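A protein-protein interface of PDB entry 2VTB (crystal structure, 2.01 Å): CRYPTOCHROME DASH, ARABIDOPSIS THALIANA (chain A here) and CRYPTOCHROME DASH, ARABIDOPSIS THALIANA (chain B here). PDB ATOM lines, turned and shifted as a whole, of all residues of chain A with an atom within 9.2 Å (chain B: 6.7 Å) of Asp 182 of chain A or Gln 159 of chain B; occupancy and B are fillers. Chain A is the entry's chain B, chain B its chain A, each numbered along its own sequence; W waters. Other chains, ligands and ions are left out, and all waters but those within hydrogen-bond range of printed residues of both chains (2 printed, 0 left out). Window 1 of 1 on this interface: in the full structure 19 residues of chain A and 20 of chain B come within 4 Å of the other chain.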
ATOM      1  N   ASP A  57      10.318  13.720 -31.835  1.00  0.00           N
ATOM      2  CA  ASP A  57      11.507  13.651 -32.692  1.00  0.00           C
ATOM      3  C   ASP A  57      11.332  12.729 -33.897  1.00  0.00           C
ATOM      4  O   ASP A  57      11.965  12.944 -34.925  1.00  0.00           O
ATOM      5  CB  ASP A  57      12.745  13.224 -31.886  1.00  0.00           C
ATOM      6  CG  ASP A  57      13.394  14.382 -31.136  1.00  0.00           C
ATOM      7  OD1 ASP A  57      13.122  15.546 -31.473  1.00  0.00           O
ATOM      8  OD2 ASP A  57      14.206  14.130 -30.220  1.00  0.00           O
ATOM      9  N   LYS A  61      11.872  14.371 -37.561  1.00  0.00           N
ATOM     10  CA  LYS A  61      12.829  13.759 -38.489  1.00  0.00           C
ATOM     11  C   LYS A  61      12.143  13.266 -39.773  1.00  0.00           C
ATOM     12  O   LYS A  61      12.667  13.462 -40.867  1.00  0.00           O
ATOM     13  CB  LYS A  61      13.615  12.629 -37.809  1.00  0.00           C
ATOM     14  CG  LYS A  61      14.567  13.121 -36.704  1.00  0.00           C
ATOM     15  CD  LYS A  61      15.256  11.970 -35.973  1.00  0.00           C
ATOM     16  CE  LYS A  61      15.972  12.435 -34.702  1.00  0.00           C
ATOM     17  NZ  LYS A  61      17.119  13.341 -34.995  1.00  0.00           N
ATOM     18  N   LEU A 172      14.731   3.940 -36.259  1.00  0.00           N
ATOM     19  CA  LEU A 172      14.232   3.967 -34.883  1.00  0.00           C
ATOM     20  C   LEU A 172      14.914   5.061 -34.058  1.00  0.00           C
ATOM     21  O   LEU A 172      16.141   5.108 -33.965  1.00  0.00           O
ATOM     22  CB  LEU A 172      14.414   2.603 -34.210  1.00  0.00           C
ATOM     23  CG  LEU A 172      13.611   1.464 -34.860  1.00  0.00           C
ATOM     24  CD1 LEU A 172      13.975   0.115 -34.256  1.00  0.00           C
ATOM     25  CD2 LEU A 172      12.106   1.718 -34.738  1.00  0.00           C
ATOM     26  N   ILE A 173      14.101   5.919 -33.448  1.00  0.00           N
ATOM     27  CA  ILE A 173      14.569   7.117 -32.764  1.00  0.00           C
ATOM     28  C   ILE A 173      14.354   6.985 -31.255  1.00  0.00           C
ATOM     29  O   ILE A 173      13.274   6.595 -30.814  1.00  0.00           O
ATOM     30  CB  ILE A 173      13.791   8.357 -33.277  1.00  0.00           C
ATOM     31  CG1 ILE A 173      13.853   8.451 -34.812  1.00  0.00           C
ATOM     32  CG2 ILE A 173      14.302   9.645 -32.625  1.00  0.00           C
ATOM     33  CD1 ILE A 173      15.260   8.470 -35.399  1.00  0.00           C
ATOM     34  N   TRP A 174      15.370   7.309 -30.463  1.00  0.00           N
ATOM     35  CA  TRP A 174      15.215   7.279 -29.014  1.00  0.00           C
ATOM     36  C   TRP A 174      14.274   8.392 -28.576  1.00  0.00           C
ATOM     37  O   TRP A 174      14.389   9.519 -29.033  1.00  0.00           O
ATOM     38  CB  TRP A 174      16.552   7.423 -28.282  1.00  0.00           C
ATOM     39  CG  TRP A 174      16.359   7.289 -26.808  1.00  0.00           C
ATOM     40  CD1 TRP A 174      16.270   8.300 -25.891  1.00  0.00           C
ATOM     41  CD2 TRP A 174      16.141   6.075 -26.089  1.00  0.00           C
ATOM     42  NE1 TRP A 174      16.045   7.783 -24.641  1.00  0.00           N
ATOM     43  CE2 TRP A 174      15.952   6.420 -24.734  1.00  0.00           C
ATOM     44  CE3 TRP A 174      16.098   4.723 -26.456  1.00  0.00           C
ATOM     45  CZ2 TRP A 174      15.730   5.466 -23.747  1.00  0.00           C
ATOM     46  CZ3 TRP A 174      15.871   3.774 -25.473  1.00  0.00           C
ATOM     47  CH2 TRP A 174      15.692   4.151 -24.132  1.00  0.00           C
ATOM     48  N   GLY A 175      13.339   8.063 -27.696  1.00  0.00           N
ATOM     49  CA  GLY A 175      12.503   9.072 -27.051  1.00  0.00           C
ATOM     50  C   GLY A 175      12.040   8.583 -25.697  1.00  0.00           C
ATOM     51  O   GLY A 175      12.682   7.744 -25.092  1.00  0.00           O
ATOM     52  N   THR A 177      12.203   9.398 -22.604  1.00  0.00           N
ATOM     53  CA  THR A 177      12.867   9.790 -21.351  1.00  0.00           C
ATOM     54  C   THR A 177      13.188  11.281 -21.207  1.00  0.00           C
ATOM     55  O   THR A 177      13.303  12.007 -22.192  1.00  0.00           O
ATOM     56  CB  THR A 177      14.164   8.976 -21.149  1.00  0.00           C
ATOM     57  OG1 THR A 177      15.056   9.192 -22.250  1.00  0.00           O
ATOM     58  CG2 THR A 177      13.853   7.499 -21.048  1.00  0.00           C
ATOM     59  N   TYR A 179      16.055  12.479 -19.495  1.00  0.00           N
ATOM     60  CA  TYR A 179      17.460  12.466 -19.891  1.00  0.00           C
ATOM     61  C   TYR A 179      17.633  11.509 -21.085  1.00  0.00           C
ATOM     62  O   TYR A 179      17.142  10.384 -21.071  1.00  0.00           O
ATOM     63  CB  TYR A 179      18.351  12.071 -18.706  1.00  0.00           C
ATOM     64  CG  TYR A 179      18.433  13.127 -17.614  1.00  0.00           C
ATOM     65  CD1 TYR A 179      17.606  13.071 -16.488  1.00  0.00           C
ATOM     66  CD2 TYR A 179      19.331  14.192 -17.710  1.00  0.00           C
ATOM     67  CE1 TYR A 179      17.674  14.048 -15.485  1.00  0.00           C
ATOM     68  CE2 TYR A 179      19.413  15.162 -16.713  1.00  0.00           C
ATOM     69  CZ  TYR A 179      18.580  15.085 -15.603  1.00  0.00           C
ATOM     70  OH  TYR A 179      18.657  16.045 -14.617  1.00  0.00           O
ATOM     71  N   HIS A 180      18.310  11.976 -22.128  1.00  0.00           N
ATOM     72  CA  HIS A 180      18.474  11.203 -23.363  1.00  0.00           C
ATOM     73  C   HIS A 180      19.535  10.115 -23.171  1.00  0.00           C
ATOM     74  O   HIS A 180      20.580  10.357 -22.571  1.00  0.00           O
ATOM     75  CB  HIS A 180      18.875  12.139 -24.508  1.00  0.00           C
ATOM     76  CG  HIS A 180      18.651  11.570 -25.877  1.00  0.00           C
ATOM     77  ND1 HIS A 180      19.475  10.614 -26.433  1.00  0.00           N
ATOM     78  CD2 HIS A 180      17.705  11.838 -26.808  1.00  0.00           C
ATOM     79  CE1 HIS A 180      19.045  10.321 -27.649  1.00  0.00           C
ATOM     80  NE2 HIS A 180      17.972  11.049 -27.899  1.00  0.00           N
ATOM     81  N   LYS A 181      19.254   8.915 -23.672  1.00  0.00           N
ATOM     82  CA  LYS A 181      20.198   7.795 -23.608  1.00  0.00           C
ATOM     83  C   LYS A 181      21.614   8.161 -24.061  1.00  0.00           C
ATOM     84  O   LYS A 181      22.595   7.785 -23.422  1.00  0.00           O
ATOM     85  CB  LYS A 181      19.701   6.634 -24.467  1.00  0.00           C
ATOM     86  CG  LYS A 181      20.467   5.339 -24.232  1.00  0.00           C
ATOM     87  CD  LYS A 181      19.734   4.121 -24.793  1.00  0.00           C
ATOM     88  CE  LYS A 181      20.106   3.844 -26.232  1.00  0.00           C
ATOM     89  NZ  LYS A 181      21.474   3.249 -26.324  1.00  0.00           N
ATOM     90  N   ASP A 182      21.699   8.874 -25.181  1.00  0.00           N
ATOM     91  CA  ASP A 182      22.984   9.279 -25.772  1.00  0.00           C
ATOM     92  C   ASP A 182      23.774  10.286 -24.927  1.00  0.00           C
ATOM     93  O   ASP A 182      24.969  10.478 -25.168  1.00  0.00           O
ATOM     94  CB  ASP A 182      22.770   9.903 -27.155  1.00  0.00           C
ATOM     95  CG  ASP A 182      22.223   8.922 -28.178  1.00  0.00           C
ATOM     96  OD1 ASP A 182      22.169   7.709 -27.902  1.00  0.00           O
ATOM     97  OD2 ASP A 182      21.839   9.390 -29.269  1.00  0.00           O
ATOM     98  N   ASP A 183      23.109  10.930 -23.969  1.00  0.00           N
ATOM     99  CA  ASP A 183      23.729  11.946 -23.111  1.00  0.00           C
ATOM    100  C   ASP A 183      24.207  11.417 -21.754  1.00  0.00           C
ATOM    101  O   ASP A 183      24.863  12.149 -21.004  1.00  0.00           O
ATOM    102  CB  ASP A 183      22.746  13.092 -22.850  1.00  0.00           C
ATOM    103  CG  ASP A 183      22.369  13.854 -24.103  1.00  0.00           C
ATOM    104  OD1 ASP A 183      23.024  13.680 -25.154  1.00  0.00           O
ATOM    105  OD2 ASP A 183      21.396  14.643 -24.035  1.00  0.00           O
ATOM    106  N   LEU A 184      23.889  10.167 -21.425  1.00  0.00           N
ATOM    107  CA  LEU A 184      24.203   9.632 -20.097  1.00  0.00           C
ATOM    108  C   LEU A 184      25.712   9.554 -19.863  1.00  0.00           C
ATOM    109  O   LEU A 184      26.472   9.402 -20.812  1.00  0.00           O
ATOM    110  CB  LEU A 184      23.603   8.233 -19.909  1.00  0.00           C
ATOM    111  CG  LEU A 184      22.081   8.095 -19.914  1.00  0.00           C
ATOM    112  CD1 LEU A 184      21.687   6.631 -19.740  1.00  0.00           C
ATOM    113  CD2 LEU A 184      21.432   8.955 -18.825  1.00  0.00           C
ATOM    114  N   PRO A 185      26.142   9.624 -18.589  1.00  0.00           N
ATOM    115  CA  PRO A 185      27.553   9.496 -18.238  1.00  0.00           C
ATOM    116  C   PRO A 185      28.024   8.037 -18.142  1.00  0.00           C
ATOM    117  O   PRO A 185      29.099   7.773 -17.611  1.00  0.00           O
ATOM    118  CB  PRO A 185      27.638  10.199 -16.881  1.00  0.00           C
ATOM    119  CG  PRO A 185      26.294  10.043 -16.284  1.00  0.00           C
ATOM    120  CD  PRO A 185      25.302   9.827 -17.392  1.00  0.00           C
ATOM    121  N   PHE A 186      27.215   7.109 -18.649  1.00  0.00           N
ATOM    122  CA  PHE A 186      27.570   5.688 -18.708  1.00  0.00           C
ATOM    123  C   PHE A 186      26.715   5.013 -19.773  1.00  0.00           C
ATOM    124  O   PHE A 186      25.632   5.505 -20.092  1.00  0.00           O
ATOM    125  CB  PHE A 186      27.362   5.006 -17.339  1.00  0.00           C
ATOM    126  CG  PHE A 186      26.286   5.644 -16.487  1.00  0.00           C
ATOM    127  CD1 PHE A 186      24.957   5.666 -16.907  1.00  0.00           C
ATOM    128  CD2 PHE A 186      26.606   6.229 -15.271  1.00  0.00           C
ATOM    129  CE1 PHE A 186      23.973   6.261 -16.127  1.00  0.00           C
ATOM    130  CE2 PHE A 186      25.626   6.833 -14.483  1.00  0.00           C
ATOM    131  CZ  PHE A 186      24.308   6.849 -14.915  1.00  0.00           C
ATOM    132  N   ASP A 187      27.203   3.916 -20.356  1.00  0.00           N
ATOM    133  CA  ASP A 187      26.349   3.093 -21.215  1.00  0.00           C
ATOM    134  C   ASP A 187      25.394   2.342 -20.300  1.00  0.00           C
ATOM    135  O   ASP A 187      25.712   2.092 -19.130  1.00  0.00           O
ATOM    136  CB  ASP A 187      27.129   2.100 -22.089  1.00  0.00           C
ATOM    137  CG  ASP A 187      26.207   1.343 -23.066  1.00  0.00           C
ATOM    138  OD1 ASP A 187      25.740   1.973 -24.053  1.00  0.00           O
ATOM    139  OD2 ASP A 187      25.909   0.139 -22.826  1.00  0.00           O
ATOM    140  N   VAL A 188      24.228   1.995 -20.834  1.00  0.00           N
ATOM    141  CA  VAL A 188      23.169   1.392 -20.034  1.00  0.00           C
ATOM    142  C   VAL A 188      23.558   0.029 -19.452  1.00  0.00           C
ATOM    143  O   VAL A 188      23.036  -0.367 -18.416  1.00  0.00           O
ATOM    144  CB  VAL A 188      21.829   1.308 -20.815  1.00  0.00           C
ATOM    145  CG1 VAL A 188      21.369   2.716 -21.219  1.00  0.00           C
ATOM    146  CG2 VAL A 188      21.951   0.400 -22.033  1.00  0.00           C
ATOM    147  N   LYS A 205      26.011  15.573 -14.187  1.00  0.00           N
ATOM    148  CA  LYS A 205      26.740  15.479 -15.463  1.00  0.00           C
ATOM    149  C   LYS A 205      25.921  15.662 -16.752  1.00  0.00           C
ATOM    150  O   LYS A 205      26.506  15.735 -17.838  1.00  0.00           O
ATOM    151  CB  LYS A 205      27.473  14.136 -15.533  1.00  0.00           C
ATOM    152  CG  LYS A 205      28.542  13.958 -14.448  1.00  0.00           C
ATOM    153  CD  LYS A 205      29.175  12.575 -14.509  1.00  0.00           C
ATOM    154  CE  LYS A 205      30.312  12.433 -13.497  1.00  0.00           C
ATOM    155  NZ  LYS A 205      30.995  11.103 -13.608  1.00  0.00           N
ATOM    156  N   CYS A 206      24.594  15.727 -16.657  1.00  0.00           N
ATOM    157  CA  CYS A 206      23.749  15.830 -17.857  1.00  0.00           C
ATOM    158  C   CYS A 206      22.884  17.075 -17.869  1.00  0.00           C
ATOM    159  O   CYS A 206      22.492  17.581 -16.813  1.00  0.00           O
ATOM    160  CB  CYS A 206      22.820  14.619 -17.977  1.00  0.00           C
ATOM    161  SG  CYS A 206      23.662  13.060 -17.937  1.00  0.00           S
ATOM    162  N   SER A 207      22.581  17.543 -19.077  1.00  0.00           N
ATOM    163  CA  SER A 207      21.569  18.563 -19.296  1.00  0.00           C
ATOM    164  C   SER A 207      20.307  17.901 -19.833  1.00  0.00           C
ATOM    165  O   SER A 207      20.377  16.896 -20.552  1.00  0.00           O
ATOM    166  CB  SER A 207      22.059  19.602 -20.312  1.00  0.00           C
ATOM    167  OG  SER A 207      23.219  20.265 -19.838  1.00  0.00           O
ATOM    168  N   ARG A 209      17.478  18.176 -22.476  1.00  0.00           N
ATOM    169  CA  ARG A 209      17.375  18.869 -23.754  1.00  0.00           C
ATOM    170  C   ARG A 209      16.098  19.693 -23.791  1.00  0.00           C
ATOM    171  O   ARG A 209      15.111  19.350 -23.136  1.00  0.00           O
ATOM    172  CB  ARG A 209      17.373  17.873 -24.914  1.00  0.00           C
ATOM    173  CG  ARG A 209      18.663  17.087 -25.083  1.00  0.00           C
ATOM    174  CD  ARG A 209      18.530  16.077 -26.204  1.00  0.00           C
ATOM    175  NE  ARG A 209      19.772  15.332 -26.398  1.00  0.00           N
ATOM    176  CZ  ARG A 209      20.010  14.505 -27.418  1.00  0.00           C
ATOM    177  NH1 ARG A 209      19.106  14.305 -28.370  1.00  0.00           N
ATOM    178  NH2 ARG A 209      21.177  13.882 -27.492  1.00  0.00           N
ATOM    179  N   PHE A 335      15.697   2.740 -18.426  1.00  0.00           N
ATOM    180  CA  PHE A 335      17.077   2.344 -18.710  1.00  0.00           C
ATOM    181  C   PHE A 335      17.396   0.997 -18.080  1.00  0.00           C
ATOM    182  O   PHE A 335      18.110   0.202 -18.677  1.00  0.00           O
ATOM    183  CB  PHE A 335      18.075   3.404 -18.227  1.00  0.00           C
ATOM    184  CG  PHE A 335      17.988   4.712 -18.970  1.00  0.00           C
ATOM    185  CD1 PHE A 335      18.062   4.753 -20.358  1.00  0.00           C
ATOM    186  CD2 PHE A 335      17.875   5.901 -18.286  1.00  0.00           C
ATOM    187  CE1 PHE A 335      17.987   5.957 -21.046  1.00  0.00           C
ATOM    188  CE2 PHE A 335      17.801   7.121 -18.971  1.00  0.00           C
ATOM    189  CZ  PHE A 335      17.860   7.147 -20.346  1.00  0.00           C
ATOM    190  N   ILE A 338      16.587  -2.110 -20.173  1.00  0.00           N
ATOM    191  CA  ILE A 338      17.617  -2.490 -21.135  1.00  0.00           C
ATOM    192  C   ILE A 338      18.716  -3.304 -20.455  1.00  0.00           C
ATOM    193  O   ILE A 338      19.161  -4.324 -20.986  1.00  0.00           O
ATOM    194  CB  ILE A 338      18.252  -1.260 -21.812  1.00  0.00           C
ATOM    195  CG1 ILE A 338      17.182  -0.417 -22.519  1.00  0.00           C
ATOM    196  CG2 ILE A 338      19.324  -1.703 -22.808  1.00  0.00           C
ATOM    197  CD1 ILE A 338      17.703   0.885 -23.092  1.00  0.00           C
ATOM    198  N   PRO B 129      37.507  13.133 -32.452  1.00  0.00           N
ATOM    199  CA  PRO B 129      36.890  14.456 -32.597  1.00  0.00           C
ATOM    200  C   PRO B 129      37.847  15.519 -33.140  1.00  0.00           C
ATOM    201  O   PRO B 129      37.435  16.376 -33.916  1.00  0.00           O
ATOM    202  CB  PRO B 129      36.472  14.808 -31.161  1.00  0.00           C
ATOM    203  CG  PRO B 129      36.361  13.498 -30.471  1.00  0.00           C
ATOM    204  CD  PRO B 129      37.432  12.652 -31.062  1.00  0.00           C
ATOM    205  N   GLU B 154      32.576   3.774 -27.401  1.00  0.00           N
ATOM    206  CA  GLU B 154      31.628   4.268 -28.418  1.00  0.00           C
ATOM    207  C   GLU B 154      30.852   5.484 -27.908  1.00  0.00           C
ATOM    208  O   GLU B 154      30.696   6.473 -28.626  1.00  0.00           O
ATOM    209  CB  GLU B 154      30.638   3.176 -28.835  1.00  0.00           C
ATOM    210  CG  GLU B 154      31.241   2.037 -29.644  1.00  0.00           C
ATOM    211  CD  GLU B 154      30.310   0.842 -29.764  1.00  0.00           C
ATOM    212  OE1 GLU B 154      29.158   0.896 -29.266  1.00  0.00           O
ATOM    213  OE2 GLU B 154      30.736  -0.166 -30.357  1.00  0.00           O
ATOM    214  N   ARG B 155      30.364   5.396 -26.672  1.00  0.00           N
ATOM    215  CA  ARG B 155      29.664   6.518 -26.025  1.00  0.00           C
ATOM    216  C   ARG B 155      30.549   7.766 -25.942  1.00  0.00           C
ATOM    217  O   ARG B 155      30.124   8.866 -26.300  1.00  0.00           O
ATOM    218  CB  ARG B 155      29.199   6.118 -24.620  1.00  0.00           C
ATOM    219  CG  ARG B 155      28.557   7.251 -23.803  1.00  0.00           C
ATOM    220  CD  ARG B 155      28.251   6.818 -22.380  1.00  0.00           C
ATOM    221  NE  ARG B 155      29.459   6.592 -21.574  1.00  0.00           N
ATOM    222  CZ  ARG B 155      30.107   7.531 -20.879  1.00  0.00           C
ATOM    223  NH1 ARG B 155      29.704   8.799 -20.881  1.00  0.00           N
ATOM    224  NH2 ARG B 155      31.184   7.203 -20.174  1.00  0.00           N
ATOM    225  N   LEU B 156      31.778   7.583 -25.469  1.00  0.00           N
ATOM    226  CA  LEU B 156      32.692   8.703 -25.272  1.00  0.00           C
ATOM    227  C   LEU B 156      33.062   9.365 -26.603  1.00  0.00           C
ATOM    228  O   LEU B 156      33.134  10.590 -26.687  1.00  0.00           O
ATOM    229  CB  LEU B 156      33.942   8.251 -24.514  1.00  0.00           C
ATOM    230  CG  LEU B 156      33.736   7.935 -23.028  1.00  0.00           C
ATOM    231  CD1 LEU B 156      34.929   7.163 -22.475  1.00  0.00           C
ATOM    232  CD2 LEU B 156      33.478   9.207 -22.205  1.00  0.00           C
ATOM    233  N   VAL B 157      33.264   8.559 -27.641  1.00  0.00           N
ATOM    234  CA  VAL B 157      33.521   9.090 -28.988  1.00  0.00           C
ATOM    235  C   VAL B 157      32.310   9.869 -29.520  1.00  0.00           C
ATOM    236  O   VAL B 157      32.454  10.980 -30.031  1.00  0.00           O
ATOM    237  CB  VAL B 157      33.878   7.965 -29.983  1.00  0.00           C
ATOM    238  CG1 VAL B 157      33.945   8.508 -31.427  1.00  0.00           C
ATOM    239  CG2 VAL B 157      35.194   7.285 -29.577  1.00  0.00           C
ATOM    240  N   ASN B 158      31.123   9.280 -29.400  1.00  0.00           N
ATOM    241  CA  ASN B 158      29.888   9.932 -29.840  1.00  0.00           C
ATOM    242  C   ASN B 158      29.651  11.260 -29.114  1.00  0.00           C
ATOM    243  O   ASN B 158      29.280  12.261 -29.736  1.00  0.00           O
ATOM    244  CB  ASN B 158      28.679   9.008 -29.641  1.00  0.00           C
ATOM    245  CG  ASN B 158      27.485   9.411 -30.494  1.00  0.00           C
ATOM    246  OD1 ASN B 158      27.639   9.777 -31.662  1.00  0.00           O
ATOM    247  ND2 ASN B 158      26.286   9.343 -29.915  1.00  0.00           N
ATOM    248  N   GLN B 159      29.869  11.266 -27.801  1.00  0.00           N
ATOM    249  CA  GLN B 159      29.724  12.488 -27.013  1.00  0.00           C
ATOM    250  C   GLN B 159      30.819  13.499 -27.371  1.00  0.00           C
ATOM    251  O   GLN B 159      30.566  14.699 -27.423  1.00  0.00           O
ATOM    252  CB  GLN B 159      29.693  12.165 -25.516  1.00  0.00           C
ATOM    253  CG  GLN B 159      28.404  11.423 -25.106  1.00  0.00           C
ATOM    254  CD  GLN B 159      28.325  11.060 -23.625  1.00  0.00           C
ATOM    255  OE1 GLN B 159      29.286  11.229 -22.869  1.00  0.00           O
ATOM    256  NE2 GLN B 159      27.163  10.549 -23.208  1.00  0.00           N
ATOM    257  N   GLY B 160      32.017  12.999 -27.664  1.00  0.00           N
ATOM    258  CA  GLY B 160      33.128  13.833 -28.114  1.00  0.00           C
ATOM    259  C   GLY B 160      32.851  14.563 -29.415  1.00  0.00           C
ATOM    260  O   GLY B 160      33.136  15.756 -29.530  1.00  0.00           O
ATOM    261  N   LEU B 161      32.291  13.856 -30.391  1.00  0.00           N
ATOM    262  CA  LEU B 161      31.958  14.457 -31.689  1.00  0.00           C
ATOM    263  C   LEU B 161      30.874  15.517 -31.513  1.00  0.00           C
ATOM    264  O   LEU B 161      30.931  16.589 -32.115  1.00  0.00           O
ATOM    265  CB  LEU B 161      31.497  13.387 -32.689  1.00  0.00           C
ATOM    266  CG  LEU B 161      32.560  12.385 -33.160  1.00  0.00           C
ATOM    267  CD1 LEU B 161      31.909  11.231 -33.924  1.00  0.00           C
ATOM    268  CD2 LEU B 161      33.634  13.051 -34.016  1.00  0.00           C
ATOM    269  N   LYS B 162      29.901  15.209 -30.665  1.00  0.00           N
ATOM    270  CA  LYS B 162      28.814  16.126 -30.330  1.00  0.00           C
ATOM    271  C   LYS B 162      29.359  17.433 -29.760  1.00  0.00           C
ATOM    272  O   LYS B 162      28.906  18.519 -30.118  1.00  0.00           O
ATOM    273  CB  LYS B 162      27.878  15.463 -29.311  1.00  0.00           C
ATOM    274  CG  LYS B 162      26.437  15.941 -29.347  1.00  0.00           C
ATOM    275  CD  LYS B 162      25.484  14.906 -28.730  1.00  0.00           C
ATOM    276  CE  LYS B 162      25.388  13.623 -29.573  1.00  0.00           C
ATOM    277  NZ  LYS B 162      24.162  12.828 -29.257  1.00  0.00           N
ATOM    278  N   ARG B 163      30.352  17.312 -28.886  1.00  0.00           N
ATOM    279  CA  ARG B 163      30.910  18.452 -28.166  1.00  0.00           C
ATOM    280  C   ARG B 163      31.655  19.434 -29.082  1.00  0.00           C
ATOM    281  O   ARG B 163      31.812  20.604 -28.733  1.00  0.00           O
ATOM    282  CB  ARG B 163      31.818  17.946 -27.040  1.00  0.00           C
ATOM    283  CG  ARG B 163      32.239  18.995 -26.031  1.00  0.00           C
ATOM    284  CD  ARG B 163      32.564  18.381 -24.669  1.00  0.00           C
ATOM    285  NE  ARG B 163      33.260  17.101 -24.797  1.00  0.00           N
ATOM    286  CZ  ARG B 163      32.778  15.909 -24.434  1.00  0.00           C
ATOM    287  NH1 ARG B 163      31.577  15.775 -23.874  1.00  0.00           N
ATOM    288  NH2 ARG B 163      33.521  14.830 -24.620  1.00  0.00           N
ATOM    289  N   VAL B 164      32.100  18.971 -30.251  1.00  0.00           N
ATOM    290  CA  VAL B 164      32.684  19.870 -31.259  1.00  0.00           C
ATOM    291  C   VAL B 164      31.641  20.399 -32.256  1.00  0.00           C
ATOM    292  O   VAL B 164      31.976  21.155 -33.169  1.00  0.00           O
ATOM    293  CB  VAL B 164      33.855  19.210 -32.026  1.00  0.00           C
ATOM    294  CG1 VAL B 164      34.874  18.629 -31.045  1.00  0.00           C
ATOM    295  CG2 VAL B 164      33.355  18.146 -32.986  1.00  0.00           C
ATOM    296  N   LEU B 170      28.728   9.662 -35.488  1.00  0.00           N
ATOM    297  CA  LEU B 170      29.286   8.315 -35.368  1.00  0.00           C
ATOM    298  C   LEU B 170      28.282   7.303 -35.922  1.00  0.00           C
ATOM    299  O   LEU B 170      27.130   7.253 -35.476  1.00  0.00           O
ATOM    300  CB  LEU B 170      29.618   7.985 -33.909  1.00  0.00           C
ATOM    301  CG  LEU B 170      30.229   6.601 -33.644  1.00  0.00           C
ATOM    302  CD1 LEU B 170      31.520   6.414 -34.431  1.00  0.00           C
ATOM    303  CD2 LEU B 170      30.475   6.378 -32.158  1.00  0.00           C
HETATM  304  O   HOH W   1      21.445  11.913 -29.814  1.00  0.00           O
HETATM  305  O   HOH W   2      26.438   8.897 -26.944  1.00  0.00           O
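Gly 175 of chain A touches none of the printed residues of chain B.
Asp 182 of chain A touches just these residues of chain B: Gln 159 and Lys 162.
Printed residues of chain B within 4 Å of Asp 183 of chain A: Gln 159 (3.4 Å).
Of the printed residues of chain B, Phe 186 of chain A touches Arg 155.
Printed residues of chain B within 4 Å of Asp 187 of chain A: Arg 155 (3.7 Å).
Of the printed residues of chain B, Arg 209 of chain A touches Lys 162.
Ile 338 of chain A touches none of the printed residues of chain B.
Gln 159 of chain B touches just these residues of chain A: Asp 182 (2.9 Å), Asp 183 (3.4 Å) and Leu 184 (2.7 Å).
No residue of chain A comes within 4 Å of Gly 160 of chain B.
The nearest residue of chain B that does not touch Asp 182 of chain A is Asn 158 of chain B (4.4 Å).
Of the 23 printed residues of chain A, 7 touch a printed residue of chain B.
Among the printed residues, 9 pairs touch across the chains.
NH1 of Arg 155 of chain B lies within hydrogen-bond range of O of Leu 184 of chain A (3.3 Å).
NH2 of Arg 155 of chain B lies within hydrogen-bond range of O of Pro 185 of chain A, at 3.4 Å.
O of Asp 182 of chain A is in hydrogen-bond range of NE2 of Gln 159 of chain B, at 2.9 Å.
NE2 of Gln 159 of chain B lies within hydrogen-bond range of O of Leu 184 of chain A, at 2.7 Å.
Among the printed residues, merely in contact across the chains: Asp 182 of chain A with Lys 162 of chain B (3.9 Å), Asp 183 of chain A with Gln 159 of chain B (3.4 Å), Phe 186 of chain A with Arg 155 of chain B (3.5 Å), Asp 187 of chain A with Arg 155 of chain B (3.7 Å) and Arg 209 of chain A with Lys 162 of chain B (3.6 Å).
The guanidinium group of Arg 155 of chain B is in hydrogen-bond range of the side-chain amide oxygen of Gln 159 of chain B, 3.2 Å away.
A ring nitrogen (ND1) of His 180 of chain A is in hydrogen-bond range of the backbone NH (N) of Asp 182 of chain A (3.1 Å).
A ring nitrogen (NE2) of His 180 of chain A lies close to the guanidinium group (NH1) of Arg 209 of chain A, at 3.5 Å.
The backbone carbonyl oxygen of Asp 183 of chain A is in hydrogen-bond range of the side-chain sulfur of Cys 206 of chain A.
OD2 of Asp 183 of chain A is in salt-bridge range of NE of Arg 209 of chain A (2.9 Å).
Water W1 lies within hydrogen-bond range of the side-chain carboxylate (OD2) of Asp 182 of chain A (2.6 Å), the side-chain amino group (NZ) of Lys 162 of chain B (2.9 Å) and the guanidinium group (NH2) of Arg 209 of chain A (3.1 Å).
Water W2 lies within hydrogen-bond range of O of Asp 182 of chain A (2.8 Å) and ND2 of Asn 158 of chain B (3.0 Å).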
